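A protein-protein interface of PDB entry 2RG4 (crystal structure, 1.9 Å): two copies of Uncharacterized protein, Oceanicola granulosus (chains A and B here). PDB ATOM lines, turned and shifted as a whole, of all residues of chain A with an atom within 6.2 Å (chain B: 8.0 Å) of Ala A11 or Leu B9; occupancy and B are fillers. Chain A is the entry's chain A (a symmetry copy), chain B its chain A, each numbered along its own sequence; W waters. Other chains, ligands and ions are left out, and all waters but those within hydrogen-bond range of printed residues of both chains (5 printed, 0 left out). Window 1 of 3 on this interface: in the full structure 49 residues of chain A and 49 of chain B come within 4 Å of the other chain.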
ATOM      1  N   SER A   8     -17.686   1.379   7.460  1.00  0.00           N
ATOM      2  CA  SER A   8     -16.953   0.080   7.215  1.00  0.00           C
ATOM      3  C   SER A   8     -15.452   0.212   6.905  1.00  0.00           C
ATOM      4  O   SER A   8     -15.043   1.026   6.008  1.00  0.00           O
ATOM      5  CB  SER A   8     -17.595  -0.744   6.136  1.00  0.00           C
ATOM      6  OG  SER A   8     -18.863  -1.171   6.543  1.00  0.00           O
ATOM      7  N   LEU A   9     -14.626  -0.544   7.651  1.00  0.00           N
ATOM      8  CA  LEU A   9     -13.156  -0.391   7.553  1.00  0.00           C
ATOM      9  C   LEU A   9     -12.549  -1.777   7.391  1.00  0.00           C
ATOM     10  O   LEU A   9     -13.204  -2.770   7.758  1.00  0.00           O
ATOM     11  CB  LEU A   9     -12.586   0.296   8.799  1.00  0.00           C
ATOM     12  CG  LEU A   9     -12.937   1.743   9.127  1.00  0.00           C
ATOM     13  CD1 LEU A   9     -12.119   2.358  10.326  1.00  0.00           C
ATOM     14  CD2 LEU A   9     -12.696   2.651   7.938  1.00  0.00           C
ATOM     15  N   PHE A  10     -11.354  -1.842   6.787  1.00  0.00           N
ATOM     16  CA  PHE A  10     -10.518  -3.040   6.869  1.00  0.00           C
ATOM     17  C   PHE A  10     -11.308  -4.283   6.326  1.00  0.00           C
ATOM     18  O   PHE A  10     -11.280  -5.371   6.918  1.00  0.00           O
ATOM     19  CB  PHE A  10      -9.960  -3.244   8.330  1.00  0.00           C
ATOM     20  CG  PHE A  10      -9.484  -1.963   9.060  1.00  0.00           C
ATOM     21  CD1 PHE A  10      -8.632  -1.053   8.444  1.00  0.00           C
ATOM     22  CD2 PHE A  10      -9.926  -1.694  10.350  1.00  0.00           C
ATOM     23  CE1 PHE A  10      -8.154   0.036   9.036  1.00  0.00           C
ATOM     24  CE2 PHE A  10      -9.423  -0.543  11.033  1.00  0.00           C
ATOM     25  CZ  PHE A  10      -8.596   0.349  10.353  1.00  0.00           C
ATOM     26  N   ALA A  11     -11.912  -4.145   5.152  1.00  0.00           N
ATOM     27  CA  ALA A  11     -12.792  -5.220   4.654  1.00  0.00           C
ATOM     28  C   ALA A  11     -11.985  -6.264   3.848  1.00  0.00           C
ATOM     29  O   ALA A  11     -11.059  -5.912   3.051  1.00  0.00           O
ATOM     30  CB  ALA A  11     -13.844  -4.625   3.745  1.00  0.00           C
ATOM     31  N   THR A  12     -12.377  -7.522   4.013  1.00  0.00           N
ATOM     32  CA  THR A  12     -11.828  -8.629   3.225  1.00  0.00           C
ATOM     33  C   THR A  12     -12.605  -8.610   1.929  1.00  0.00           C
ATOM     34  O   THR A  12     -13.788  -8.256   1.950  1.00  0.00           O
ATOM     35  CB  THR A  12     -12.081  -9.936   4.049  1.00  0.00           C
ATOM     36  OG1 THR A  12     -11.215  -9.885   5.185  1.00  0.00           O
ATOM     37  CG2 THR A  12     -11.780 -11.270   3.270  1.00  0.00           C
ATOM     38  N   ARG A  13     -11.933  -8.891   0.786  1.00  0.00           N
ATOM     39  CA  ARG A  13     -12.639  -9.007  -0.498  1.00  0.00           C
ATOM     40  C   ARG A  13     -12.634 -10.494  -0.971  1.00  0.00           C
ATOM     41  O   ARG A  13     -11.617 -11.164  -0.833  1.00  0.00           O
ATOM     42  CB  ARG A  13     -12.015  -8.060  -1.546  1.00  0.00           C
ATOM     43  CG  ARG A  13     -11.911  -6.585  -1.081  1.00  0.00           C
ATOM     44  CD  ARG A  13     -13.309  -6.000  -1.187  1.00  0.00           C
ATOM     45  NE  ARG A  13     -13.561  -5.710  -2.621  1.00  0.00           N
ATOM     46  CZ  ARG A  13     -14.722  -5.295  -3.101  1.00  0.00           C
ATOM     47  NH1 ARG A  13     -15.807  -5.099  -2.313  1.00  0.00           N
ATOM     48  NH2 ARG A  13     -14.788  -5.024  -4.369  1.00  0.00           N
ATOM     49  N   LEU A  14     -13.805 -11.011  -1.373  1.00  0.00           N
ATOM     50  CA  LEU A  14     -13.981 -12.336  -1.992  1.00  0.00           C
ATOM     51  C   LEU A  14     -14.309 -12.102  -3.499  1.00  0.00           C
ATOM     52  O   LEU A  14     -15.231 -11.363  -3.872  1.00  0.00           O
ATOM     53  CB  LEU A  14     -15.172 -13.117  -1.371  1.00  0.00           C
ATOM     54  CG  LEU A  14     -15.362 -14.527  -1.983  1.00  0.00           C
ATOM     55  CD1 LEU A  14     -14.032 -15.361  -1.784  1.00  0.00           C
ATOM     56  CD2 LEU A  14     -16.545 -15.156  -1.300  1.00  0.00           C
ATOM     57  N   LEU A  91      -7.879  -5.217  -5.024  1.00  0.00           N
ATOM     58  CA  LEU A  91      -7.315  -5.159  -3.650  1.00  0.00           C
ATOM     59  C   LEU A  91      -6.356  -3.986  -3.447  1.00  0.00           C
ATOM     60  O   LEU A  91      -5.934  -3.759  -2.354  1.00  0.00           O
ATOM     61  CB  LEU A  91      -6.596  -6.456  -3.245  1.00  0.00           C
ATOM     62  CG  LEU A  91      -7.511  -7.652  -3.029  1.00  0.00           C
ATOM     63  CD1 LEU A  91      -6.588  -8.840  -3.222  1.00  0.00           C
ATOM     64  CD2 LEU A  91      -8.192  -7.611  -1.585  1.00  0.00           C
ATOM     65  N   LEU A 143     -15.725 -19.565   4.420  1.00  0.00           N
ATOM     66  CA  LEU A 143     -14.648 -18.639   4.823  1.00  0.00           C
ATOM     67  C   LEU A 143     -14.926 -18.139   6.208  1.00  0.00           C
ATOM     68  O   LEU A 143     -16.090 -17.841   6.546  1.00  0.00           O
ATOM     69  CB  LEU A 143     -14.595 -17.399   3.871  1.00  0.00           C
ATOM     70  CG  LEU A 143     -14.325 -17.511   2.360  1.00  0.00           C
ATOM     71  CD1 LEU A 143     -13.222 -18.400   2.075  1.00  0.00           C
ATOM     72  CD2 LEU A 143     -15.476 -18.039   1.610  1.00  0.00           C
ATOM     73  N   ARG A 147     -10.849 -12.144  12.041  1.00  0.00           N
ATOM     74  CA  ARG A 147     -10.885 -11.557  13.375  1.00  0.00           C
ATOM     75  C   ARG A 147     -11.547 -12.480  14.380  1.00  0.00           C
ATOM     76  O   ARG A 147     -11.689 -12.086  15.528  1.00  0.00           O
ATOM     77  CB  ARG A 147     -11.668 -10.206  13.408  1.00  0.00           C
ATOM     78  CG  ARG A 147     -11.106  -9.148  12.477  1.00  0.00           C
ATOM     79  CD  ARG A 147     -12.120  -8.048  12.234  1.00  0.00           C
ATOM     80  NE  ARG A 147     -13.342  -8.664  11.654  1.00  0.00           N
ATOM     81  CZ  ARG A 147     -14.515  -8.063  11.659  1.00  0.00           C
ATOM     82  NH1 ARG A 147     -14.622  -6.837  12.149  1.00  0.00           N
ATOM     83  NH2 ARG A 147     -15.580  -8.669  11.168  1.00  0.00           N
ATOM     84  N   GLU A 163     -24.274  -8.868   4.799  1.00  0.00           N
ATOM     85  CA  GLU A 163     -23.243  -9.874   4.654  1.00  0.00           C
ATOM     86  C   GLU A 163     -21.861  -9.413   5.152  1.00  0.00           C
ATOM     87  O   GLU A 163     -21.036 -10.232   5.550  1.00  0.00           O
ATOM     88  CB  GLU A 163     -23.170 -10.361   3.205  1.00  0.00           C
ATOM     89  CG  GLU A 163     -23.481  -9.317   2.084  1.00  0.00           C
ATOM     90  CD  GLU A 163     -24.095 -10.001   0.842  1.00  0.00           C
ATOM     91  OE1 GLU A 163     -23.908 -11.229   0.733  1.00  0.00           O
ATOM     92  OE2 GLU A 163     -24.773  -9.345   0.025  1.00  0.00           O
ATOM     93  N   GLU A 164     -21.598  -8.105   5.128  1.00  0.00           N
ATOM     94  CA  GLU A 164     -20.275  -7.687   5.587  1.00  0.00           C
ATOM     95  C   GLU A 164     -20.126  -7.771   7.096  1.00  0.00           C
ATOM     96  O   GLU A 164     -19.008  -7.641   7.627  1.00  0.00           O
ATOM     97  CB  GLU A 164     -19.846  -6.307   5.024  1.00  0.00           C
ATOM     98  CG  GLU A 164     -19.951  -5.189   5.978  1.00  0.00           C
ATOM     99  CD  GLU A 164     -20.972  -4.209   5.546  1.00  0.00           C
ATOM    100  OE1 GLU A 164     -20.656  -2.989   5.561  1.00  0.00           O
ATOM    101  OE2 GLU A 164     -22.084  -4.674   5.152  1.00  0.00           O
ATOM    102  N   LEU A 165     -21.224  -7.952   7.833  1.00  0.00           N
ATOM    103  CA  LEU A 165     -21.070  -8.158   9.243  1.00  0.00           C
ATOM    104  C   LEU A 165     -21.077  -9.608   9.717  1.00  0.00           C
ATOM    105  O   LEU A 165     -21.078  -9.879  10.933  1.00  0.00           O
ATOM    106  CB  LEU A 165     -22.165  -7.421   9.998  1.00  0.00           C
ATOM    107  CG  LEU A 165     -22.245  -5.959   9.675  1.00  0.00           C
ATOM    108  CD1 LEU A 165     -23.622  -5.484   9.994  1.00  0.00           C
ATOM    109  CD2 LEU A 165     -21.258  -5.366  10.528  1.00  0.00           C
ATOM    110  N   ARG A 166     -21.137 -10.543   8.799  1.00  0.00           N
ATOM    111  CA  ARG A 166     -21.339 -11.937   9.185  1.00  0.00           C
ATOM    112  C   ARG A 166     -20.015 -12.555   9.464  1.00  0.00           C
ATOM    113  O   ARG A 166     -19.021 -12.150   8.831  1.00  0.00           O
ATOM    114  CB  ARG A 166     -21.952 -12.719   8.041  1.00  0.00           C
ATOM    115  CG  ARG A 166     -23.421 -12.256   7.602  1.00  0.00           C
ATOM    116  CD  ARG A 166     -24.411 -12.780   8.650  1.00  0.00           C
ATOM    117  NE  ARG A 166     -24.368 -14.214   8.541  1.00  0.00           N
ATOM    118  CZ  ARG A 166     -25.121 -14.886   7.667  1.00  0.00           C
ATOM    119  NH1 ARG A 166     -25.993 -14.243   6.904  1.00  0.00           N
ATOM    120  NH2 ARG A 166     -25.037 -16.189   7.580  1.00  0.00           N
ATOM    121  N   ARG A 169     -18.754 -16.808   5.928  1.00  0.00           N
ATOM    122  CA  ARG A 169     -19.389 -16.723   4.648  1.00  0.00           C
ATOM    123  C   ARG A 169     -19.296 -18.117   3.893  1.00  0.00           C
ATOM    124  O   ARG A 169     -18.203 -18.625   3.653  1.00  0.00           O
ATOM    125  CB  ARG A 169     -18.619 -15.714   3.838  1.00  0.00           C
ATOM    126  CG  ARG A 169     -19.137 -15.660   2.365  1.00  0.00           C
ATOM    127  CD  ARG A 169     -20.583 -15.090   2.220  1.00  0.00           C
ATOM    128  NE  ARG A 169     -20.660 -14.361   0.943  1.00  0.00           N
ATOM    129  CZ  ARG A 169     -20.810 -14.926  -0.235  1.00  0.00           C
ATOM    130  NH1 ARG A 169     -20.948 -16.247  -0.365  1.00  0.00           N
ATOM    131  NH2 ARG A 169     -20.797 -14.169  -1.296  1.00  0.00           N
ATOM    132  N   GLU A 182      -7.341 -13.632  -0.330  1.00  0.00           N
ATOM    133  CA  GLU A 182      -6.010 -13.460   0.141  1.00  0.00           C
ATOM    134  C   GLU A 182      -5.601 -14.691   0.999  1.00  0.00           C
ATOM    135  O   GLU A 182      -6.398 -15.127   1.837  1.00  0.00           O
ATOM    136  CB  GLU A 182      -5.918 -12.135   0.931  1.00  0.00           C
ATOM    137  CG  GLU A 182      -5.540 -10.946   0.020  1.00  0.00           C
ATOM    138  CD  GLU A 182      -5.223  -9.659   0.846  1.00  0.00           C
ATOM    139  OE1 GLU A 182      -4.057  -9.483   1.403  1.00  0.00           O
ATOM    140  OE2 GLU A 182      -6.211  -8.869   0.941  1.00  0.00           O
ATOM    141  N   LEU A 185      -6.501 -15.987   4.610  1.00  0.00           N
ATOM    142  CA  LEU A 185      -7.874 -16.161   5.014  1.00  0.00           C
ATOM    143  C   LEU A 185      -8.179 -17.659   5.229  1.00  0.00           C
ATOM    144  O   LEU A 185      -7.891 -18.516   4.359  1.00  0.00           O
ATOM    145  CB  LEU A 185      -8.831 -15.660   3.929  1.00  0.00           C
ATOM    146  CG  LEU A 185     -10.352 -15.678   4.239  1.00  0.00           C
ATOM    147  CD1 LEU A 185     -10.780 -14.610   5.332  1.00  0.00           C
ATOM    148  CD2 LEU A 185     -11.083 -15.298   2.973  1.00  0.00           C
ATOM    149  N   ILE B   6     -17.275  -9.176  -6.846  1.00  0.00           N
ATOM    150  CA  ILE B   6     -16.252  -9.096  -5.764  1.00  0.00           C
ATOM    151  C   ILE B   6     -16.983  -8.495  -4.565  1.00  0.00           C
ATOM    152  O   ILE B   6     -17.509  -7.405  -4.683  1.00  0.00           O
ATOM    153  CB  ILE B   6     -14.984  -8.188  -6.077  1.00  0.00           C
ATOM    154  CG1 ILE B   6     -14.486  -8.372  -7.517  1.00  0.00           C
ATOM    155  CG2 ILE B   6     -13.903  -8.403  -5.048  1.00  0.00           C
ATOM    156  CD1 ILE B   6     -13.103  -7.759  -7.819  1.00  0.00           C
ATOM    157  N   LYS B   7     -16.962  -9.186  -3.422  1.00  0.00           N
ATOM    158  CA  LYS B   7     -17.753  -8.868  -2.234  1.00  0.00           C
ATOM    159  C   LYS B   7     -16.873  -8.460  -1.055  1.00  0.00           C
ATOM    160  O   LYS B   7     -15.772  -8.986  -0.870  1.00  0.00           O
ATOM    161  CB  LYS B   7     -18.622 -10.054  -1.805  1.00  0.00           C
ATOM    162  CG  LYS B   7     -19.337 -10.796  -2.813  1.00  0.00           C
ATOM    163  CD  LYS B   7     -20.426  -9.967  -3.403  1.00  0.00           C
ATOM    164  CE  LYS B   7     -21.449  -9.559  -2.386  1.00  0.00           C
ATOM    165  NZ  LYS B   7     -22.310  -8.592  -3.129  1.00  0.00           N
ATOM    166  N   SER B   8     -17.290  -7.415  -0.364  1.00  0.00           N
ATOM    167  CA  SER B   8     -16.735  -7.047   0.992  1.00  0.00           C
ATOM    168  C   SER B   8     -17.230  -7.906   2.169  1.00  0.00           C
ATOM    169  O   SER B   8     -18.480  -8.112   2.340  1.00  0.00           O
ATOM    170  CB  SER B   8     -16.956  -5.600   1.326  1.00  0.00           C
ATOM    171  OG  SER B   8     -16.225  -4.785   0.457  1.00  0.00           O
ATOM    172  N   LEU B   9     -16.277  -8.435   2.957  1.00  0.00           N
ATOM    173  CA  LEU B   9     -16.621  -9.400   4.026  1.00  0.00           C
ATOM    174  C   LEU B   9     -15.932  -8.951   5.305  1.00  0.00           C
ATOM    175  O   LEU B   9     -14.942  -8.199   5.226  1.00  0.00           O
ATOM    176  CB  LEU B   9     -16.177 -10.819   3.653  1.00  0.00           C
ATOM    177  CG  LEU B   9     -16.809 -11.557   2.478  1.00  0.00           C
ATOM    178  CD1 LEU B   9     -16.384 -13.069   2.350  1.00  0.00           C
ATOM    179  CD2 LEU B   9     -18.321 -11.546   2.571  1.00  0.00           C
ATOM    180  N   PHE B  10     -16.489  -9.345   6.459  1.00  0.00           N
ATOM    181  CA  PHE B  10     -15.761  -9.277   7.725  1.00  0.00           C
ATOM    182  C   PHE B  10     -15.288  -7.805   7.994  1.00  0.00           C
ATOM    183  O   PHE B  10     -14.147  -7.561   8.410  1.00  0.00           O
ATOM    184  CB  PHE B  10     -14.583 -10.326   7.760  1.00  0.00           C
ATOM    185  CG  PHE B  10     -14.900 -11.722   7.168  1.00  0.00           C
ATOM    186  CD1 PHE B  10     -16.049 -12.418   7.528  1.00  0.00           C
ATOM    187  CD2 PHE B  10     -14.037 -12.295   6.240  1.00  0.00           C
ATOM    188  CE1 PHE B  10     -16.348 -13.636   7.089  1.00  0.00           C
ATOM    189  CE2 PHE B  10     -14.310 -13.612   5.755  1.00  0.00           C
ATOM    190  CZ  PHE B  10     -15.494 -14.247   6.129  1.00  0.00           C
ATOM    191  N   ALA B  11     -16.200  -6.848   7.862  1.00  0.00           N
ATOM    192  CA  ALA B  11     -15.791  -5.434   7.954  1.00  0.00           C
ATOM    193  C   ALA B  11     -15.833  -4.942   9.419  1.00  0.00           C
ATOM    194  O   ALA B  11     -16.772  -5.284  10.204  1.00  0.00           O
ATOM    195  CB  ALA B  11     -16.739  -4.583   7.138  1.00  0.00           C
ATOM    196  N   THR B  12     -14.859  -4.104   9.755  1.00  0.00           N
ATOM    197  CA  THR B  12     -14.817  -3.423  11.053  1.00  0.00           C
ATOM    198  C   THR B  12     -15.726  -2.225  10.896  1.00  0.00           C
ATOM    199  O   THR B  12     -15.797  -1.673   9.794  1.00  0.00           O
ATOM    200  CB  THR B  12     -13.327  -3.010  11.295  1.00  0.00           C
ATOM    201  OG1 THR B  12     -12.597  -4.214  11.537  1.00  0.00           O
ATOM    202  CG2 THR B  12     -13.105  -2.054  12.526  1.00  0.00           C
ATOM    203  N   ASP B 145      -5.563  -1.628  10.836  1.00  0.00           N
ATOM    204  CA  ASP B 145      -6.126  -2.912  10.364  1.00  0.00           C
ATOM    205  C   ASP B 145      -5.711  -4.104  11.310  1.00  0.00           C
ATOM    206  O   ASP B 145      -4.531  -4.349  11.578  1.00  0.00           O
ATOM    207  CB  ASP B 145      -5.678  -3.172   8.895  1.00  0.00           C
ATOM    208  CG  ASP B 145      -6.526  -4.174   8.174  1.00  0.00           C
ATOM    209  OD1 ASP B 145      -7.041  -5.127   8.775  1.00  0.00           O
ATOM    210  OD2 ASP B 145      -6.635  -4.050   6.936  1.00  0.00           O
ATOM    211  N   PRO B 146      -6.720  -4.795  11.883  1.00  0.00           N
ATOM    212  CA  PRO B 146      -6.589  -5.918  12.797  1.00  0.00           C
ATOM    213  C   PRO B 146      -5.890  -7.038  12.043  1.00  0.00           C
ATOM    214  O   PRO B 146      -5.223  -7.870  12.628  1.00  0.00           O
ATOM    215  CB  PRO B 146      -8.032  -6.194  13.172  1.00  0.00           C
ATOM    216  CG  PRO B 146      -8.855  -5.609  12.047  1.00  0.00           C
ATOM    217  CD  PRO B 146      -8.126  -4.393  11.720  1.00  0.00           C
ATOM    218  N   ARG B 147      -5.978  -6.999  10.702  1.00  0.00           N
ATOM    219  CA  ARG B 147      -5.333  -8.026   9.893  1.00  0.00           C
ATOM    220  C   ARG B 147      -3.902  -7.658   9.552  1.00  0.00           C
ATOM    221  O   ARG B 147      -3.262  -8.411   8.832  1.00  0.00           O
ATOM    222  CB  ARG B 147      -6.078  -8.273   8.543  1.00  0.00           C
ATOM    223  CG  ARG B 147      -7.527  -8.691   8.709  1.00  0.00           C
ATOM    224  CD  ARG B 147      -8.295  -8.504   7.416  1.00  0.00           C
ATOM    225  NE  ARG B 147      -8.201  -7.073   7.023  1.00  0.00           N
ATOM    226  CZ  ARG B 147      -8.443  -6.652   5.798  1.00  0.00           C
ATOM    227  NH1 ARG B 147      -8.839  -7.515   4.875  1.00  0.00           N
ATOM    228  NH2 ARG B 147      -8.306  -5.376   5.489  1.00  0.00           N
ATOM    229  N   MET B 151      -0.853  -9.836   7.235  1.00  0.00           N
ATOM    230  CA  MET B 151      -0.444  -9.327   5.911  1.00  0.00           C
ATOM    231  C   MET B 151       1.037  -9.209   5.638  1.00  0.00           C
ATOM    232  O   MET B 151       1.444  -8.418   4.778  1.00  0.00           O
ATOM    233  CB  MET B 151      -1.142  -8.003   5.609  1.00  0.00           C
ATOM    234  CG  MET B 151      -2.654  -8.087   5.494  1.00  0.00           C
ATOM    235  SD  MET B 151      -3.548  -6.517   5.592  1.00  0.00           S
ATOM    236  CE  MET B 151      -2.767  -5.577   6.830  1.00  0.00           C
ATOM    237  N   ARG B 157      -0.623  -1.681   0.248  1.00  0.00           N
ATOM    238  CA  ARG B 157      -1.747  -1.217  -0.540  1.00  0.00           C
ATOM    239  C   ARG B 157      -1.664   0.249  -0.869  1.00  0.00           C
ATOM    240  O   ARG B 157      -1.236   1.041  -0.025  1.00  0.00           O
ATOM    241  CB  ARG B 157      -2.970  -1.386   0.304  1.00  0.00           C
ATOM    242  CG  ARG B 157      -2.752  -2.471   1.286  1.00  0.00           C
ATOM    243  CD  ARG B 157      -3.384  -3.673   0.760  1.00  0.00           C
ATOM    244  NE  ARG B 157      -4.775  -3.481   1.076  1.00  0.00           N
ATOM    245  CZ  ARG B 157      -5.676  -4.443   1.171  1.00  0.00           C
ATOM    246  NH1 ARG B 157      -6.892  -4.097   1.521  1.00  0.00           N
ATOM    247  NH2 ARG B 157      -5.351  -5.718   0.963  1.00  0.00           N
ATOM    248  N   GLU B 163     -12.012   3.777   1.168  1.00  0.00           N
ATOM    249  CA  GLU B 163     -11.601   3.742   2.555  1.00  0.00           C
ATOM    250  C   GLU B 163     -11.678   2.339   3.183  1.00  0.00           C
ATOM    251  O   GLU B 163     -10.949   2.035   4.125  1.00  0.00           O
ATOM    252  CB  GLU B 163     -12.402   4.755   3.376  1.00  0.00           C
ATOM    253  CG  GLU B 163     -13.886   5.006   2.951  1.00  0.00           C
ATOM    254  CD  GLU B 163     -14.323   6.450   3.286  1.00  0.00           C
ATOM    255  OE1 GLU B 163     -13.644   7.053   4.141  1.00  0.00           O
ATOM    256  OE2 GLU B 163     -15.284   6.978   2.690  1.00  0.00           O
ATOM    257  N   GLU B 164     -12.560   1.478   2.673  1.00  0.00           N
ATOM    258  CA  GLU B 164     -12.633   0.157   3.292  1.00  0.00           C
ATOM    259  C   GLU B 164     -11.448  -0.723   2.933  1.00  0.00           C
ATOM    260  O   GLU B 164     -11.256  -1.798   3.531  1.00  0.00           O
ATOM    261  CB  GLU B 164     -13.991  -0.552   3.054  1.00  0.00           C
ATOM    262  CG  GLU B 164     -13.966  -1.613   2.031  1.00  0.00           C
ATOM    263  CD  GLU B 164     -14.800  -1.253   0.863  1.00  0.00           C
ATOM    264  OE1 GLU B 164     -15.603  -2.121   0.428  1.00  0.00           O
ATOM    265  OE2 GLU B 164     -14.673  -0.076   0.408  1.00  0.00           O
ATOM    266  N   LEU B 165     -10.642  -0.330   1.944  1.00  0.00           N
ATOM    267  CA  LEU B 165      -9.455  -1.092   1.690  1.00  0.00           C
ATOM    268  C   LEU B 165      -8.169  -0.566   2.319  1.00  0.00           C
ATOM    269  O   LEU B 165      -7.070  -1.089   2.049  1.00  0.00           O
ATOM    270  CB  LEU B 165      -9.222  -1.207   0.191  1.00  0.00           C
ATOM    271  CG  LEU B 165     -10.391  -1.766  -0.562  1.00  0.00           C
ATOM    272  CD1 LEU B 165     -10.291  -1.320  -1.982  1.00  0.00           C
ATOM    273  CD2 LEU B 165     -10.235  -3.185  -0.430  1.00  0.00           C
ATOM    274  N   ARG B 166      -8.265   0.481   3.102  1.00  0.00           N
ATOM    275  CA  ARG B 166      -7.059   1.150   3.582  1.00  0.00           C
ATOM    276  C   ARG B 166      -6.606   0.486   4.834  1.00  0.00           C
ATOM    277  O   ARG B 166      -7.463  -0.020   5.586  1.00  0.00           O
ATOM    278  CB  ARG B 166      -7.359   2.592   3.939  1.00  0.00           C
ATOM    279  CG  ARG B 166      -7.817   3.520   2.716  1.00  0.00           C
ATOM    280  CD  ARG B 166      -6.569   3.858   1.891  1.00  0.00           C
ATOM    281  NE  ARG B 166      -5.742   4.665   2.750  1.00  0.00           N
ATOM    282  CZ  ARG B 166      -5.891   5.987   2.846  1.00  0.00           C
ATOM    283  NH1 ARG B 166      -6.781   6.616   2.090  1.00  0.00           N
ATOM    284  NH2 ARG B 166      -5.137   6.685   3.656  1.00  0.00           N
HETATM  285  O   HOH W   1     -11.689  -8.271   7.023  1.00  0.00           O
HETATM  286  O   HOH W   2     -18.549 -11.101   6.484  1.00  0.00           O
HETATM  287  O   HOH W   3      -9.974   0.405   6.175  1.00  0.00           O
HETATM  288  O   HOH W   4      -3.111  -6.661   2.026  1.00  0.00           O
HETATM  289  O   HOH W   5     -12.171  -5.793   9.657  1.00  0.00           O
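Of the 17 printed residues of chain A, 15 touch a printed residue of chain B.
Hydrophobic or aromatic side chains of chain A that line the printed part of chain B: Leu A9, Phe A10, Ala A11, Leu A14, Leu A143 and Leu A185.
Hydrophobic or aromatic side chains of chain B that line the printed part of chain A: Ile B6, Leu B9, Phe B10, Ala B11, Pro B146 and Leu B165.
Among the printed residues, pairs that only touch across the chains: Leu A14 with Ile B6 (3.1 Å), Arg A13 with Lys B7 (3.2 Å), Phe A10 with Arg B166 (3.3 Å), Arg A166 with Phe B10 (3.3 Å), Ser A8 with Thr B12 (3.3 Å), Thr A12 with Ser B8 (3.3 Å), Phe A10 with Asp B145 (3.5 Å), Ser A8 with Glu B164 (3.5 Å), Glu A164 with Ser B8 (3.5 Å), Phe A10 with Pro B146 (3.5 Å), Thr A12 with Lys B7 (3.5 Å), Arg A13 with Ile B6 (3.6 Å), Leu A91 with Arg B157 (3.6 Å), Leu A143 with Phe B10 (3.7 Å), Leu A185 with Phe B10 (3.7 Å), Ala A11 with Leu B9 (3.7 Å), Leu A9 with Ala B11 (3.7 Å), Thr A12 with Phe B10 (3.8 Å), Phe A10 with Thr B12 (3.8 Å), Arg A169 with Leu B9 (3.8 Å), Arg A13 with Leu B165 (3.8 Å), Phe A10 with Phe B10 (3.9 Å), Leu A14 with Leu B9 (3.9 Å) and Arg A169 with Lys B7 (3.98 Å).
Water W1 lies within hydrogen-bond range of the side-chain hydroxyl of Thr A12, the backbone carbonyl oxygen of Phe B10 and the backbone carbonyl oxygen of Phe A10.
Water W5 lies within hydrogen-bond range of OG1 of Thr B12, O of Phe A10 and O of Phe B10.
Water W2 lies within hydrogen-bond range of the backbone carbonyl oxygen of Arg A166 (2.6 Å), the backbone NH of Phe B10 (2.7 Å) and the backbone carbonyl oxygen of Glu A163 (2.8 Å).
Water W3 lies within hydrogen-bond range of O of Arg B166 (2.6 Å), N of Phe A10 (2.7 Å) and O of Glu B163 (2.8 Å).
Leu A9 touches Ala B11, and with the chains exchanged Ala A11 touches Leu B9.
Phe B10 touches its own counterpart, Phe A10.
Phe A10 touches Glu B164, and with the chains exchanged Glu A164 touches Phe B10.
Ala A11 touches Arg B147, and with the chains exchanged Arg A147 touches Ala B11.
Of the 39 pairs that touch across the chains among the printed residues, 23 have their exchanged pair printed and touching as well.
O of Thr B12 lies within hydrogen-bond range of N of Leu A9, at 2.7 Å.
The guanidinium group (NH2) of Arg A147 sits at hydrogen-bond distance from the backbone carbonyl oxygen (O) of Phe B10 (3.3 Å).
The backbone carbonyl oxygen (O) of Thr A12 is in hydrogen-bond range of the backbone NH (N) of Leu B9 (2.7 Å).
OE2 of Glu A182 lies within salt-bridge range of NH2 of Arg B157 (3.3 Å).
N of Lys B7 is in hydrogen-bond range of O of Leu A14, 2.8 Å away.
The guanidinium group of Arg B147 lies within hydrogen-bond range of the backbone carbonyl oxygen of Ala A11 (3.3 Å).
OG1 of Thr A12 sits at hydrogen-bond distance from NH1 of Arg B147 (3.4 Å).
N of Ala B11 is in hydrogen-bond range of O of Glu A164, 2.9 Å away.
NH1 of Arg A147 lies within hydrogen-bond range of O of Ala B11.
The backbone NH (N) of Ala A11 is in hydrogen-bond range of the backbone carbonyl oxygen (O) of Glu B164 (2.9 Å).
The backbone NH (N) of Phe A10 is in hydrogen-bond range of the backbone carbonyl oxygen (O) of Glu B164, 3.3 Å away.
The guanidinium group of Arg B147 sits at hydrogen-bond distance from the backbone carbonyl oxygen of Phe A10 (3.3 Å).
NH1 of Arg A13 is in hydrogen-bond range of OG of Ser B8 (2.8 Å).
The guanidinium group (NH1) of Arg A147 sits at hydrogen-bond distance from the side-chain hydroxyl (OG1) of Thr B12 (3.4 Å).
N of Phe B10 lies within hydrogen-bond range of O of Glu A164 (3.3 Å).
Of chain A, only Ala A11 (3.7 Å), Thr A12 (2.7 Å), Leu A14 (3.9 Å) and Arg A169 (3.8 Å) come within 4 Å of Leu B9.
Printed residues of chain B within 4 Å of Leu A14: Ile B6 (3.1 Å), Lys B7 (2.8 Å) and Leu B9 (3.9 Å).
Printed residues of chain B within 4 Å of Leu A185: Phe B10.
Glu A163 touches none of the printed residues of chain B.
The side-chain hydroxyl of Ser A8 is in hydrogen-bond range of the side-chain carboxylate of Glu A164, 2.7 Å away.
The backbone carbonyl oxygen (O) of Leu B165 lies within hydrogen-bond range of the guanidinium group (NH1) of Arg B157 (3.1 Å).
The guanidinium group (NH2) of Arg B147 lies within salt-bridge range of the side-chain carboxylate (OD2) of Asp B145 (2.6 Å).
The backbone NH (N) of Leu A143 is in hydrogen-bond range of the backbone carbonyl oxygen (O) of Arg A169 (2.8 Å).
The side-chain carboxylate of Glu B164 is in hydrogen-bond range of the side-chain hydroxyl of Ser B8, at 2.7 Å.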
